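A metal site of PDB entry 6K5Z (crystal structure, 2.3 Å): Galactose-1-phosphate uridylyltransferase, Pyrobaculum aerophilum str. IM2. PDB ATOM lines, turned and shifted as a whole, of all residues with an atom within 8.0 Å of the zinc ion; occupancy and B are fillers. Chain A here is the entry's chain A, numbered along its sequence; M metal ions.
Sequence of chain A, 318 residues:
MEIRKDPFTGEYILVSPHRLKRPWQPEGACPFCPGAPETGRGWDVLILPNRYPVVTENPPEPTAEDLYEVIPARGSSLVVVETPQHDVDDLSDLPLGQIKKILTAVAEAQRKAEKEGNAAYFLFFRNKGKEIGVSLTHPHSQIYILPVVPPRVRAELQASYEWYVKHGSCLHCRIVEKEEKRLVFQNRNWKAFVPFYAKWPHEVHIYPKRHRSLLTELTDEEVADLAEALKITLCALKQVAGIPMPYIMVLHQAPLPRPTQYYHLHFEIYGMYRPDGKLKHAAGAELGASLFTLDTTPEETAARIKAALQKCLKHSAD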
ATOM      1  N   GLY A  28       0.842  -3.308  19.584  1.00  0.00           N
ATOM      2  CA  GLY A  28       0.852  -3.811  18.189  1.00  0.00           C
ATOM      3  C   GLY A  28       2.245  -4.032  17.586  1.00  0.00           C
ATOM      4  O   GLY A  28       2.384  -4.124  16.356  1.00  0.00           O
ATOM      5  N   ALA A  29       3.276  -4.063  18.453  1.00  0.00           N
ATOM      6  CA  ALA A  29       4.666  -4.332  18.046  1.00  0.00           C
ATOM      7  C   ALA A  29       4.934  -5.781  18.370  1.00  0.00           C
ATOM      8  O   ALA A  29       4.635  -6.245  19.482  1.00  0.00           O
ATOM      9  CB  ALA A  29       5.675  -3.451  18.794  1.00  0.00           C
ATOM     10  N   CYS A  30       5.441  -6.486  17.377  1.00  0.00           N
ATOM     11  CA  CYS A  30       5.805  -7.853  17.510  1.00  0.00           C
ATOM     12  C   CYS A  30       7.309  -7.941  17.416  1.00  0.00           C
ATOM     13  O   CYS A  30       7.895  -7.500  16.415  1.00  0.00           O
ATOM     14  CB  CYS A  30       5.151  -8.692  16.411  1.00  0.00           C
ATOM     15  SG  CYS A  30       5.666 -10.456  16.372  1.00  0.00           S
ATOM     16  N   PRO A  31       7.945  -8.500  18.451  1.00  0.00           N
ATOM     17  CA  PRO A  31       9.368  -8.669  18.487  1.00  0.00           C
ATOM     18  C   PRO A  31       9.909  -9.779  17.545  1.00  0.00           C
ATOM     19  O   PRO A  31      11.128  -9.919  17.393  1.00  0.00           O
ATOM     20  CB  PRO A  31       9.616  -9.058  19.927  1.00  0.00           C
ATOM     21  CG  PRO A  31       8.388  -9.813  20.320  1.00  0.00           C
ATOM     22  CD  PRO A  31       7.258  -9.278  19.507  1.00  0.00           C
ATOM     23  N   PHE A  32       9.030 -10.572  16.952  1.00  0.00           N
ATOM     24  CA  PHE A  32       9.431 -11.604  15.996  1.00  0.00           C
ATOM     25  C   PHE A  32       9.078 -11.254  14.562  1.00  0.00           C
ATOM     26  O   PHE A  32       9.476 -11.950  13.637  1.00  0.00           O
ATOM     27  CB  PHE A  32       8.767 -12.945  16.344  1.00  0.00           C
ATOM     28  CG  PHE A  32       8.886 -13.346  17.788  1.00  0.00           C
ATOM     29  CD1 PHE A  32      10.105 -13.191  18.484  1.00  0.00           C
ATOM     30  CD2 PHE A  32       7.806 -13.928  18.446  1.00  0.00           C
ATOM     31  CE1 PHE A  32      10.219 -13.571  19.812  1.00  0.00           C
ATOM     32  CE2 PHE A  32       7.916 -14.329  19.753  1.00  0.00           C
ATOM     33  CZ  PHE A  32       9.111 -14.147  20.446  1.00  0.00           C
ATOM     34  N   CYS A  33       8.317 -10.178  14.377  1.00  0.00           N
ATOM     35  CA  CYS A  33       8.011  -9.683  13.044  1.00  0.00           C
ATOM     36  C   CYS A  33       9.217  -9.139  12.250  1.00  0.00           C
ATOM     37  O   CYS A  33      10.168  -8.538  12.838  1.00  0.00           O
ATOM     38  CB  CYS A  33       6.946  -8.620  13.118  1.00  0.00           C
ATOM     39  SG  CYS A  33       5.401  -9.343  12.691  1.00  0.00           S
ATOM     40  N   PRO A  34       9.208  -9.373  10.924  1.00  0.00           N
ATOM     41  CA  PRO A  34      10.296  -8.793  10.134  1.00  0.00           C
ATOM     42  C   PRO A  34      10.281  -7.249  10.227  1.00  0.00           C
ATOM     43  O   PRO A  34       9.204  -6.656  10.224  1.00  0.00           O
ATOM     44  CB  PRO A  34      10.001  -9.319   8.702  1.00  0.00           C
ATOM     45  CG  PRO A  34       8.524  -9.582   8.668  1.00  0.00           C
ATOM     46  CD  PRO A  34       8.227 -10.078  10.066  1.00  0.00           C
ATOM     47  N   TRP A  43      14.280 -12.878   5.229  1.00  0.00           N
ATOM     48  CA  TRP A  43      14.489 -14.143   5.936  1.00  0.00           C
ATOM     49  C   TRP A  43      13.227 -14.965   5.929  1.00  0.00           C
ATOM     50  O   TRP A  43      12.118 -14.412   5.867  1.00  0.00           O
ATOM     51  CB  TRP A  43      14.952 -13.927   7.367  1.00  0.00           C
ATOM     52  CG  TRP A  43      14.057 -13.034   8.249  1.00  0.00           C
ATOM     53  CD1 TRP A  43      14.229 -11.711   8.487  1.00  0.00           C
ATOM     54  CD2 TRP A  43      12.931 -13.451   9.021  1.00  0.00           C
ATOM     55  NE1 TRP A  43      13.255 -11.261   9.350  1.00  0.00           N
ATOM     56  CE2 TRP A  43      12.442 -12.308   9.686  1.00  0.00           C
ATOM     57  CE3 TRP A  43      12.278 -14.657   9.205  1.00  0.00           C
ATOM     58  CZ2 TRP A  43      11.342 -12.345  10.540  1.00  0.00           C
ATOM     59  CZ3 TRP A  43      11.158 -14.680  10.036  1.00  0.00           C
ATOM     60  CH2 TRP A  43      10.726 -13.539  10.698  1.00  0.00           C
ATOM     61  N   VAL A  81      11.619 -18.296  15.254  1.00  0.00           N
ATOM     62  CA  VAL A  81      10.566 -17.601  14.542  1.00  0.00           C
ATOM     63  C   VAL A  81      10.378 -18.435  13.288  1.00  0.00           C
ATOM     64  O   VAL A  81      11.280 -18.554  12.472  1.00  0.00           O
ATOM     65  CB  VAL A  81      10.911 -16.146  14.199  1.00  0.00           C
ATOM     66  CG1 VAL A  81       9.678 -15.421  13.703  1.00  0.00           C
ATOM     67  CG2 VAL A  81      11.399 -15.431  15.426  1.00  0.00           C
ATOM     68  N   THR A  83       8.308 -18.281  10.672  1.00  0.00           N
ATOM     69  CA  THR A  83       7.784 -17.656   9.445  1.00  0.00           C
ATOM     70  C   THR A  83       7.834 -16.109   9.603  1.00  0.00           C
ATOM     71  O   THR A  83       7.778 -15.619  10.723  1.00  0.00           O
ATOM     72  CB  THR A  83       6.329 -18.098   9.157  1.00  0.00           C
ATOM     73  OG1 THR A  83       5.778 -17.323   8.088  1.00  0.00           O
ATOM     74  CG2 THR A  83       5.455 -17.928  10.344  1.00  0.00           C
ATOM     75  N   PRO A  84       7.936 -15.349   8.493  1.00  0.00           N
ATOM     76  CA  PRO A  84       7.843 -13.874   8.604  1.00  0.00           C
ATOM     77  C   PRO A  84       6.429 -13.371   8.782  1.00  0.00           C
ATOM     78  O   PRO A  84       6.232 -12.243   9.222  1.00  0.00           O
ATOM     79  CB  PRO A  84       8.374 -13.357   7.250  1.00  0.00           C
ATOM     80  CG  PRO A  84       8.898 -14.537   6.532  1.00  0.00           C
ATOM     81  CD  PRO A  84       8.209 -15.761   7.101  1.00  0.00           C
ATOM     82  N   GLN A  85       5.465 -14.201   8.447  1.00  0.00           N
ATOM     83  CA  GLN A  85       4.079 -13.818   8.518  1.00  0.00           C
ATOM     84  C   GLN A  85       3.572 -13.822   9.956  1.00  0.00           C
ATOM     85  O   GLN A  85       3.710 -14.819  10.664  1.00  0.00           O
ATOM     86  CB  GLN A  85       3.228 -14.775   7.641  1.00  0.00           C
ATOM     87  CG  GLN A  85       3.585 -14.775   6.146  1.00  0.00           C
ATOM     88  CD  GLN A  85       2.818 -15.833   5.379  1.00  0.00           C
ATOM     89  OE1 GLN A  85       1.578 -15.869   5.442  1.00  0.00           O
ATOM     90  NE2 GLN A  85       3.532 -16.721   4.699  1.00  0.00           N
ATOM     91  N   HIS A  86       2.951 -12.727  10.374  1.00  0.00           N
ATOM     92  CA  HIS A  86       2.395 -12.590  11.703  1.00  0.00           C
ATOM     93  C   HIS A  86       1.083 -13.357  11.914  1.00  0.00           C
ATOM     94  O   HIS A  86       0.834 -13.828  13.020  1.00  0.00           O
ATOM     95  CB  HIS A  86       2.163 -11.095  12.013  1.00  0.00           C
ATOM     96  CG  HIS A  86       1.766 -10.834  13.414  1.00  0.00           C
ATOM     97  ND1 HIS A  86       2.681 -10.708  14.432  1.00  0.00           N
ATOM     98  CD2 HIS A  86       0.543 -10.727  13.993  1.00  0.00           C
ATOM     99  CE1 HIS A  86       2.050 -10.518  15.576  1.00  0.00           C
ATOM    100  NE2 HIS A  86       0.748 -10.542  15.334  1.00  0.00           N
ATOM    101  N   ASP A  87       0.278 -13.455  10.848  1.00  0.00           N
ATOM    102  CA  ASP A  87      -1.157 -13.802  10.910  1.00  0.00           C
ATOM    103  C   ASP A  87      -1.513 -15.301  10.730  1.00  0.00           C
ATOM    104  O   ASP A  87      -2.704 -15.662  10.708  1.00  0.00           O
ATOM    105  CB  ASP A  87      -1.901 -12.983   9.833  1.00  0.00           C
ATOM    106  CG  ASP A  87      -1.590 -11.484   9.909  1.00  0.00           C
ATOM    107  OD1 ASP A  87      -1.444 -10.943  11.038  1.00  0.00           O
ATOM    108  OD2 ASP A  87      -1.454 -10.832   8.849  1.00  0.00           O
ATOM    109  N   LEU A 136       2.152 -14.184  22.716  1.00  0.00           N
ATOM    110  CA  LEU A 136       2.738 -13.766  21.411  1.00  0.00           C
ATOM    111  C   LEU A 136       2.257 -14.691  20.278  1.00  0.00           C
ATOM    112  O   LEU A 136       2.728 -15.821  20.091  1.00  0.00           O
ATOM    113  CB  LEU A 136       4.245 -13.702  21.515  1.00  0.00           C
ATOM    114  CG  LEU A 136       4.719 -12.692  22.578  1.00  0.00           C
ATOM    115  CD1 LEU A 136       6.242 -12.827  22.815  1.00  0.00           C
ATOM    116  CD2 LEU A 136       4.347 -11.241  22.212  1.00  0.00           C
ATOM    117  N   THR A 137       1.244 -14.219  19.575  1.00  0.00           N
ATOM    118  CA  THR A 137       0.533 -15.002  18.603  1.00  0.00           C
ATOM    119  C   THR A 137       1.388 -15.457  17.397  1.00  0.00           C
ATOM    120  O   THR A 137       1.050 -16.432  16.725  1.00  0.00           O
ATOM    121  CB  THR A 137      -0.639 -14.174  18.088  1.00  0.00           C
ATOM    122  OG1 THR A 137      -1.531 -15.028  17.383  1.00  0.00           O
ATOM    123  CG2 THR A 137      -0.184 -13.096  17.104  1.00  0.00           C
ATOM    124  N   HIS A 138       2.438 -14.711  17.080  1.00  0.00           N
ATOM    125  CA  HIS A 138       3.249 -14.937  15.915  1.00  0.00           C
ATOM    126  C   HIS A 138       3.908 -16.310  16.003  1.00  0.00           C
ATOM    127  O   HIS A 138       4.686 -16.513  16.913  1.00  0.00           O
ATOM    128  CB  HIS A 138       4.353 -13.854  15.790  1.00  0.00           C
ATOM    129  CG  HIS A 138       5.094 -13.895  14.476  1.00  0.00           C
ATOM    130  ND1 HIS A 138       5.621 -12.775  13.892  1.00  0.00           N
ATOM    131  CD2 HIS A 138       5.376 -14.920  13.637  1.00  0.00           C
ATOM    132  CE1 HIS A 138       6.196 -13.099  12.748  1.00  0.00           C
ATOM    133  NE2 HIS A 138       6.067 -14.399  12.581  1.00  0.00           N
ATOM    134  N   PRO A 139       3.641 -17.227  15.052  1.00  0.00           N
ATOM    135  CA  PRO A 139       4.181 -18.614  15.116  1.00  0.00           C
ATOM    136  C   PRO A 139       5.639 -18.788  15.537  1.00  0.00           C
ATOM    137  O   PRO A 139       6.550 -18.372  14.844  1.00  0.00           O
ATOM    138  CB  PRO A 139       3.977 -19.123  13.704  1.00  0.00           C
ATOM    139  CG  PRO A 139       2.657 -18.503  13.337  1.00  0.00           C
ATOM    140  CD  PRO A 139       2.621 -17.142  13.990  1.00  0.00           C
HETATM  141 ZN    ZN M   1       4.735 -10.841  14.379  1.00  0.00          ZN
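NE2 of His 138 is in hydrogen-bond range of O of Gln 85 (3.1 Å).
A ring nitrogen (NE2) of His 138 lies within hydrogen-bond range of the backbone carbonyl oxygen of Thr 83 (2.8 Å).
N of Phe 32 sits close to SG of Cys 30, 3.4 Å away.
Within 4 Å of the zinc ion: Cys 30, Cys 33, His 86 and His 138.
The nearest printed residue that does not touch the zinc ion is Phe 32 (4.4 Å).
The zinc ion is bound by ND1 of His 86 (2.1 Å).
ND1 of His 138 binds the zinc ion.
The side-chain sulfur (SG) of Cys 30 binds the zinc ion.
The zinc ion is bound by SG of Cys 33 (2.4 Å).
The zinc ion has four donor atoms within binding distance.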
